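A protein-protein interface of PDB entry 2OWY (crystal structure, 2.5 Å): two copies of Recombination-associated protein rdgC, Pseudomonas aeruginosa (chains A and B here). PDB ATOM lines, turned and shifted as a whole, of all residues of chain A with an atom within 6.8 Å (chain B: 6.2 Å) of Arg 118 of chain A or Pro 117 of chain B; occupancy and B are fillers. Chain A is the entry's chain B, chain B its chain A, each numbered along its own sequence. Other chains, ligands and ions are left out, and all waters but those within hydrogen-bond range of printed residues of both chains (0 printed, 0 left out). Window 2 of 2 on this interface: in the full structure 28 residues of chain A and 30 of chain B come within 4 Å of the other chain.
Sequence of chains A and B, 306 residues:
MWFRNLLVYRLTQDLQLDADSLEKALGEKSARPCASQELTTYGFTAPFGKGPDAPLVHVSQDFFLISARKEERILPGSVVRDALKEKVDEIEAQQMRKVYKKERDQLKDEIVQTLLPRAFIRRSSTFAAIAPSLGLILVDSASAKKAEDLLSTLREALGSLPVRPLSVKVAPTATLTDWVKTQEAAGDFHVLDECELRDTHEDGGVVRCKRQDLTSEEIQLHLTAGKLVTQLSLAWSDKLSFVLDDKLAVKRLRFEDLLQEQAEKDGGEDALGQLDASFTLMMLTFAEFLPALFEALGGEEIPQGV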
ATOM      1  N   SER A  36     -12.163  22.412 -14.431  1.00  0.00           N
ATOM      2  CA  SER A  36     -12.177  21.009 -14.012  1.00  0.00           C
ATOM      3  C   SER A  36     -11.029  20.150 -14.541  1.00  0.00           C
ATOM      4  O   SER A  36     -10.641  19.174 -13.899  1.00  0.00           O
ATOM      5  CB  SER A  36     -13.514  20.363 -14.380  1.00  0.00           C
ATOM      6  OG  SER A  36     -14.526  20.748 -13.465  1.00  0.00           O
ATOM      7  N   ARG A  73      -5.552  22.526  -8.264  1.00  0.00           N
ATOM      8  CA  ARG A  73      -6.256  21.357  -7.766  1.00  0.00           C
ATOM      9  C   ARG A  73      -5.260  20.435  -7.074  1.00  0.00           C
ATOM     10  O   ARG A  73      -4.174  20.179  -7.596  1.00  0.00           O
ATOM     11  CB  ARG A  73      -6.934  20.628  -8.925  1.00  0.00           C
ATOM     12  CG  ARG A  73      -8.012  21.449  -9.611  1.00  0.00           C
ATOM     13  CD  ARG A  73      -8.695  20.673 -10.728  1.00  0.00           C
ATOM     14  NE  ARG A  73      -9.949  21.311 -11.126  1.00  0.00           N
ATOM     15  CZ  ARG A  73     -10.989  21.480 -10.312  1.00  0.00           C
ATOM     16  NH1 ARG A  73     -10.925  21.055  -9.056  1.00  0.00           N
ATOM     17  NH2 ARG A  73     -12.090  22.078 -10.750  1.00  0.00           N
ATOM     18  N   ILE A  74      -5.618  19.956  -5.889  1.00  0.00           N
ATOM     19  CA  ILE A  74      -4.733  19.054  -5.170  1.00  0.00           C
ATOM     20  C   ILE A  74      -4.995  17.593  -5.557  1.00  0.00           C
ATOM     21  O   ILE A  74      -6.055  17.026  -5.283  1.00  0.00           O
ATOM     22  CB  ILE A  74      -4.826  19.267  -3.607  1.00  0.00           C
ATOM     23  CG1 ILE A  74      -5.155  17.957  -2.883  1.00  0.00           C
ATOM     24  CG2 ILE A  74      -5.848  20.356  -3.285  1.00  0.00           C
ATOM     25  CD1 ILE A  74      -6.654  17.626  -2.798  1.00  0.00           C
ATOM     26  N   THR A 114      -9.351  11.899 -14.913  1.00  0.00           N
ATOM     27  CA  THR A 114     -10.606  11.426 -14.336  1.00  0.00           C
ATOM     28  C   THR A 114     -10.712  11.896 -12.892  1.00  0.00           C
ATOM     29  O   THR A 114     -11.807  12.075 -12.368  1.00  0.00           O
ATOM     30  CB  THR A 114     -10.713   9.882 -14.346  1.00  0.00           C
ATOM     31  OG1 THR A 114     -10.767   9.408 -15.697  1.00  0.00           O
ATOM     32  CG2 THR A 114     -11.973   9.427 -13.610  1.00  0.00           C
ATOM     33  N   LEU A 115      -9.564  12.108 -12.256  1.00  0.00           N
ATOM     34  CA  LEU A 115      -9.534  12.541 -10.862  1.00  0.00           C
ATOM     35  C   LEU A 115      -9.549  14.056 -10.635  1.00  0.00           C
ATOM     36  O   LEU A 115     -10.060  14.514  -9.616  1.00  0.00           O
ATOM     37  CB  LEU A 115      -8.307  11.947 -10.160  1.00  0.00           C
ATOM     38  CG  LEU A 115      -8.237  10.435  -9.975  1.00  0.00           C
ATOM     39  CD1 LEU A 115      -6.854  10.053  -9.484  1.00  0.00           C
ATOM     40  CD2 LEU A 115      -9.304   9.990  -8.995  1.00  0.00           C
ATOM     41  N   LEU A 116      -8.996  14.823 -11.574  1.00  0.00           N
ATOM     42  CA  LEU A 116      -8.928  16.281 -11.441  1.00  0.00           C
ATOM     43  C   LEU A 116     -10.223  16.960 -10.995  1.00  0.00           C
ATOM     44  O   LEU A 116     -10.266  17.619  -9.951  1.00  0.00           O
ATOM     45  CB  LEU A 116      -8.445  16.911 -12.750  1.00  0.00           C
ATOM     46  CG  LEU A 116      -6.941  16.773 -12.991  1.00  0.00           C
ATOM     47  CD1 LEU A 116      -6.554  17.404 -14.319  1.00  0.00           C
ATOM     48  CD2 LEU A 116      -6.182  17.431 -11.843  1.00  0.00           C
ATOM     49  N   PRO A 117     -11.302  16.795 -11.772  1.00  0.00           N
ATOM     50  CA  PRO A 117     -12.599  17.398 -11.451  1.00  0.00           C
ATOM     51  C   PRO A 117     -13.023  17.185 -10.002  1.00  0.00           C
ATOM     52  O   PRO A 117     -13.803  17.957  -9.453  1.00  0.00           O
ATOM     53  CB  PRO A 117     -13.550  16.696 -12.412  1.00  0.00           C
ATOM     54  CG  PRO A 117     -12.679  16.379 -13.575  1.00  0.00           C
ATOM     55  CD  PRO A 117     -11.425  15.880 -12.921  1.00  0.00           C
ATOM     56  N   ARG A 118     -12.501  16.131  -9.393  1.00  0.00           N
ATOM     57  CA  ARG A 118     -12.846  15.785  -8.027  1.00  0.00           C
ATOM     58  C   ARG A 118     -11.863  16.342  -6.995  1.00  0.00           C
ATOM     59  O   ARG A 118     -12.105  16.284  -5.785  1.00  0.00           O
ATOM     60  CB  ARG A 118     -12.918  14.263  -7.923  1.00  0.00           C
ATOM     61  CG  ARG A 118     -13.184  13.732  -6.538  1.00  0.00           C
ATOM     62  CD  ARG A 118     -13.066  12.221  -6.537  1.00  0.00           C
ATOM     63  NE  ARG A 118     -13.151  11.665  -5.193  1.00  0.00           N
ATOM     64  CZ  ARG A 118     -12.934  10.385  -4.905  1.00  0.00           C
ATOM     65  NH1 ARG A 118     -12.620   9.537  -5.877  1.00  0.00           N
ATOM     66  NH2 ARG A 118     -13.023   9.958  -3.651  1.00  0.00           N
ATOM     67  N   ALA A 119     -10.763  16.903  -7.477  1.00  0.00           N
ATOM     68  CA  ALA A 119      -9.742  17.440  -6.593  1.00  0.00           C
ATOM     69  C   ALA A 119     -10.062  18.797  -5.968  1.00  0.00           C
ATOM     70  O   ALA A 119     -10.343  19.768  -6.669  1.00  0.00           O
ATOM     71  CB  ALA A 119      -8.417  17.518  -7.341  1.00  0.00           C
ATOM     72  N   PHE A 120     -10.002  18.851  -4.639  1.00  0.00           N
ATOM     73  CA  PHE A 120     -10.239  20.084  -3.904  1.00  0.00           C
ATOM     74  C   PHE A 120      -9.255  21.112  -4.445  1.00  0.00           C
ATOM     75  O   PHE A 120      -8.294  20.758  -5.126  1.00  0.00           O
ATOM     76  CB  PHE A 120      -9.973  19.868  -2.413  1.00  0.00           C
ATOM     77  CG  PHE A 120     -10.885  18.866  -1.769  1.00  0.00           C
ATOM     78  CD1 PHE A 120     -10.489  18.190  -0.618  1.00  0.00           C
ATOM     79  CD2 PHE A 120     -12.146  18.604  -2.299  1.00  0.00           C
ATOM     80  CE1 PHE A 120     -11.337  17.264  -0.001  1.00  0.00           C
ATOM     81  CE2 PHE A 120     -12.996  17.685  -1.689  1.00  0.00           C
ATOM     82  CZ  PHE A 120     -12.592  17.013  -0.538  1.00  0.00           C
ATOM     83  N   SER B  36     -17.352   6.545   3.084  1.00  0.00           N
ATOM     84  CA  SER B  36     -17.483   7.897   2.540  1.00  0.00           C
ATOM     85  C   SER B  36     -17.756   8.983   3.595  1.00  0.00           C
ATOM     86  O   SER B  36     -17.541  10.169   3.336  1.00  0.00           O
ATOM     87  CB  SER B  36     -18.562   7.932   1.443  1.00  0.00           C
ATOM     88  OG  SER B  36     -19.867   7.935   1.985  1.00  0.00           O
ATOM     89  N   GLN B  37     -18.219   8.583   4.778  1.00  0.00           N
ATOM     90  CA  GLN B  37     -18.495   9.544   5.851  1.00  0.00           C
ATOM     91  C   GLN B  37     -17.529   9.307   7.007  1.00  0.00           C
ATOM     92  O   GLN B  37     -17.701   9.861   8.095  1.00  0.00           O
ATOM     93  CB  GLN B  37     -19.930   9.391   6.372  1.00  0.00           C
ATOM     94  CG  GLN B  37     -21.043   9.517   5.329  1.00  0.00           C
ATOM     95  CD  GLN B  37     -21.009  10.826   4.545  1.00  0.00           C
ATOM     96  OE1 GLN B  37     -20.730  11.898   5.095  1.00  0.00           O
ATOM     97  NE2 GLN B  37     -21.312  10.742   3.252  1.00  0.00           N
ATOM     98  N   ARG B  73      -8.938  10.070   4.768  1.00  0.00           N
ATOM     99  CA  ARG B  73      -9.496  10.942   3.738  1.00  0.00           C
ATOM    100  C   ARG B  73      -8.796  12.302   3.758  1.00  0.00           C
ATOM    101  O   ARG B  73      -8.585  12.882   4.826  1.00  0.00           O
ATOM    102  CB  ARG B  73     -11.000  11.111   3.961  1.00  0.00           C
ATOM    103  CG  ARG B  73     -11.793   9.827   3.760  1.00  0.00           C
ATOM    104  CD  ARG B  73     -13.292  10.061   3.811  1.00  0.00           C
ATOM    105  NE  ARG B  73     -14.038   8.927   3.273  1.00  0.00           N
ATOM    106  CZ  ARG B  73     -14.061   8.592   1.986  1.00  0.00           C
ATOM    107  NH1 ARG B  73     -13.380   9.312   1.099  1.00  0.00           N
ATOM    108  NH2 ARG B  73     -14.759   7.535   1.579  1.00  0.00           N
ATOM    109  N   VAL B 112     -18.377  19.359   5.725  1.00  0.00           N
ATOM    110  CA  VAL B 112     -17.577  18.160   5.892  1.00  0.00           C
ATOM    111  C   VAL B 112     -18.360  16.970   5.350  1.00  0.00           C
ATOM    112  O   VAL B 112     -17.878  16.255   4.473  1.00  0.00           O
ATOM    113  CB  VAL B 112     -17.225  17.927   7.385  1.00  0.00           C
ATOM    114  CG1 VAL B 112     -16.608  16.551   7.572  1.00  0.00           C
ATOM    115  CG2 VAL B 112     -16.244  18.994   7.856  1.00  0.00           C
ATOM    116  N   GLN B 113     -19.571  16.781   5.865  1.00  0.00           N
ATOM    117  CA  GLN B 113     -20.441  15.684   5.444  1.00  0.00           C
ATOM    118  C   GLN B 113     -20.606  15.652   3.927  1.00  0.00           C
ATOM    119  O   GLN B 113     -20.782  14.594   3.342  1.00  0.00           O
ATOM    120  CB  GLN B 113     -21.816  15.812   6.120  1.00  0.00           C
ATOM    121  CG  GLN B 113     -22.810  14.695   5.769  1.00  0.00           C
ATOM    122  CD  GLN B 113     -24.122  14.776   6.555  1.00  0.00           C
ATOM    123  OE1 GLN B 113     -24.866  15.759   6.463  1.00  0.00           O
ATOM    124  NE2 GLN B 113     -24.409  13.735   7.328  1.00  0.00           N
ATOM    125  N   THR B 114     -20.539  16.815   3.293  1.00  0.00           N
ATOM    126  CA  THR B 114     -20.678  16.910   1.840  1.00  0.00           C
ATOM    127  C   THR B 114     -19.351  16.642   1.129  1.00  0.00           C
ATOM    128  O   THR B 114     -19.311  15.986   0.088  1.00  0.00           O
ATOM    129  CB  THR B 114     -21.157  18.323   1.408  1.00  0.00           C
ATOM    130  OG1 THR B 114     -22.428  18.601   2.001  1.00  0.00           O
ATOM    131  CG2 THR B 114     -21.276  18.414  -0.113  1.00  0.00           C
ATOM    132  N   LEU B 115     -18.266  17.150   1.699  1.00  0.00           N
ATOM    133  CA  LEU B 115     -16.958  17.000   1.093  1.00  0.00           C
ATOM    134  C   LEU B 115     -16.215  15.709   1.401  1.00  0.00           C
ATOM    135  O   LEU B 115     -15.400  15.264   0.595  1.00  0.00           O
ATOM    136  CB  LEU B 115     -16.085  18.207   1.455  1.00  0.00           C
ATOM    137  CG  LEU B 115     -16.509  19.562   0.873  1.00  0.00           C
ATOM    138  CD1 LEU B 115     -15.499  20.625   1.270  1.00  0.00           C
ATOM    139  CD2 LEU B 115     -16.607  19.472  -0.641  1.00  0.00           C
ATOM    140  N   LEU B 116     -16.473  15.100   2.552  1.00  0.00           N
ATOM    141  CA  LEU B 116     -15.784  13.858   2.868  1.00  0.00           C
ATOM    142  C   LEU B 116     -15.854  12.851   1.716  1.00  0.00           C
ATOM    143  O   LEU B 116     -14.827  12.476   1.147  1.00  0.00           O
ATOM    144  CB  LEU B 116     -16.339  13.233   4.154  1.00  0.00           C
ATOM    145  CG  LEU B 116     -15.669  13.763   5.429  1.00  0.00           C
ATOM    146  CD1 LEU B 116     -16.065  12.943   6.653  1.00  0.00           C
ATOM    147  CD2 LEU B 116     -14.176  13.697   5.245  1.00  0.00           C
ATOM    148  N   PRO B 117     -17.067  12.425   1.334  1.00  0.00           N
ATOM    149  CA  PRO B 117     -17.219  11.457   0.241  1.00  0.00           C
ATOM    150  C   PRO B 117     -16.459  11.770  -1.052  1.00  0.00           C
ATOM    151  O   PRO B 117     -16.181  10.873  -1.841  1.00  0.00           O
ATOM    152  CB  PRO B 117     -18.730  11.418   0.027  1.00  0.00           C
ATOM    153  CG  PRO B 117     -19.160  12.794   0.433  1.00  0.00           C
ATOM    154  CD  PRO B 117     -18.371  13.002   1.698  1.00  0.00           C
ATOM    155  N   ARG B 118     -16.118  13.034  -1.264  1.00  0.00           N
ATOM    156  CA  ARG B 118     -15.407  13.436  -2.477  1.00  0.00           C
ATOM    157  C   ARG B 118     -13.891  13.425  -2.281  1.00  0.00           C
ATOM    158  O   ARG B 118     -13.132  13.485  -3.248  1.00  0.00           O
ATOM    159  CB  ARG B 118     -15.854  14.844  -2.895  1.00  0.00           C
ATOM    160  CG  ARG B 118     -17.372  15.023  -2.950  1.00  0.00           C
ATOM    161  CD  ARG B 118     -17.788  16.491  -3.066  1.00  0.00           C
ATOM    162  NE  ARG B 118     -19.244  16.650  -3.106  1.00  0.00           N
ATOM    163  CZ  ARG B 118     -19.875  17.814  -3.275  1.00  0.00           C
ATOM    164  NH1 ARG B 118     -19.184  18.941  -3.421  1.00  0.00           N
ATOM    165  NH2 ARG B 118     -21.204  17.850  -3.309  1.00  0.00           N
ATOM    166  N   ALA B 119     -13.458  13.339  -1.027  1.00  0.00           N
ATOM    167  CA  ALA B 119     -12.035  13.359  -0.683  1.00  0.00           C
ATOM    168  C   ALA B 119     -11.201  12.154  -1.115  1.00  0.00           C
ATOM    169  O   ALA B 119     -11.640  11.009  -1.026  1.00  0.00           O
ATOM    170  CB  ALA B 119     -11.875  13.568   0.826  1.00  0.00           C
ATOM    171  N   PHE B 120      -9.986  12.424  -1.575  1.00  0.00           N
ATOM    172  CA  PHE B 120      -9.081  11.359  -1.975  1.00  0.00           C
ATOM    173  C   PHE B 120      -8.580  10.682  -0.701  1.00  0.00           C
ATOM    174  O   PHE B 120      -8.608  11.271   0.383  1.00  0.00           O
ATOM    175  CB  PHE B 120      -7.902  11.926  -2.766  1.00  0.00           C
ATOM    176  CG  PHE B 120      -8.292  12.534  -4.079  1.00  0.00           C
ATOM    177  CD1 PHE B 120      -7.633  13.667  -4.558  1.00  0.00           C
ATOM    178  CD2 PHE B 120      -9.309  11.971  -4.845  1.00  0.00           C
ATOM    179  CE1 PHE B 120      -7.975  14.234  -5.781  1.00  0.00           C
ATOM    180  CE2 PHE B 120      -9.661  12.530  -6.072  1.00  0.00           C
ATOM    181  CZ  PHE B 120      -8.994  13.665  -6.542  1.00  0.00           C
ATOM    182  N   ILE B 121      -8.120   9.444  -0.835  1.00  0.00           N
ATOM    183  CA  ILE B 121      -7.634   8.682   0.302  1.00  0.00           C
ATOM    184  C   ILE B 121      -6.124   8.515   0.301  1.00  0.00           C
ATOM    185  O   ILE B 121      -5.501   8.339  -0.745  1.00  0.00           O
ATOM    186  CB  ILE B 121      -8.309   7.304   0.339  1.00  0.00           C
ATOM    187  CG1 ILE B 121      -9.812   7.497   0.582  1.00  0.00           C
ATOM    188  CG2 ILE B 121      -7.668   6.426   1.404  1.00  0.00           C
ATOM    189  CD1 ILE B 121     -10.619   6.216   0.635  1.00  0.00           C
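Leu 115 of chain A touches Phe 120 of chain B, and with the chains exchanged Phe 120 of chain A touches Leu 115 of chain B.
Arg 118 of chain A touches Pro 117 of chain B, but with the chains exchanged Pro 117 of chain A does not touch Arg 118 of chain B (7.5 Å).
Arg 118 of chain A touches Ala 119 of chain B, but with the chains exchanged Ala 119 of chain A does not touch Arg 118 of chain B (5.9 Å).
Ala 119 of chain A touches Phe 120 of chain B, and with the chains exchanged Phe 120 of chain A touches Ala 119 of chain B.
9 positions are printed for both chains.
Of the 9 pairs that touch across the chains among the printed residues, 5 have their exchanged pair printed and touching as well.
Among the printed residues, pairs that only touch across the chains: Leu 115 of chain A with Phe 120 of chain B (3.4 Å), Ile 74 of chain A with Phe 120 of chain B (3.4 Å), Arg 118 of chain A with Phe 120 of chain B (3.5 Å), Phe 120 of chain A with Leu 115 of chain B (3.5 Å), Ala 119 of chain A with Phe 120 of chain B (3.7 Å), Phe 120 of chain A with Ala 119 of chain B (3.7 Å) and Arg 118 of chain A with Pro 117 of chain B (3.8 Å).
Of the 13 printed residues of chain B, 5 touch a printed residue of chain A.
Hydrophobic or aromatic side chains of chain A that line the printed part of chain B: Leu 115, Ala 119 and Phe 120.
Arg 118 of chain A touches just these residues of chain B: Pro 117 (3.8 Å), Arg 118 (2.7 Å), Ala 119 (3.1 Å) and Phe 120 (3.5 Å).
Of the printed residues of chain B, Ala 119 of chain A touches Phe 120 (3.7 Å).
Of the printed residues of chain B, Phe 120 of chain A touches Leu 115 (3.5 Å) and Ala 119 (3.7 Å).
Gln 37 of chain B touches none of the printed residues of chain A.
Printed residues of chain A within 4 Å of Leu 115 of chain B: Phe 120.
Of chain A, only Arg 118 (3.8 Å) comes within 4 Å of Pro 117 of chain B.
Printed residues of chain A within 4 Å of Arg 118 of chain B: Arg 118.
Of the printed residues of chain A, Ala 119 of chain B touches Arg 118 and Phe 120.
The nearest residue of chain B that does not touch Arg 118 of chain A is Arg 73 of chain B (4.8 Å).
The nearest printed residue of chain B that does not touch Ile 74 of chain A is Ala 119 of chain B (7.2 Å).
The backbone carbonyl oxygen (O) of Ala 119 of chain B sits at hydrogen-bond distance from the guanidinium group (NH1) of Arg 73 of chain B, at 3.2 Å.
The backbone carbonyl oxygen of Phe 120 of chain A is in hydrogen-bond range of the backbone NH of Ile 74 of chain A (2.9 Å).
The guanidinium group of Arg 73 of chain A sits at hydrogen-bond distance from the backbone carbonyl oxygen of Ala 119 of chain A.
O of Thr 114 of chain B lies within hydrogen-bond range of NE of Arg 118 of chain B (3.3 Å).
O of Ala 119 of chain B lies within hydrogen-bond range of NH2 of Arg 118 of chain A, 3.1 Å away.
The guanidinium group (NE) of Arg 118 of chain A sits at hydrogen-bond distance from the backbone carbonyl oxygen (O) of Arg 118 of chain B.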
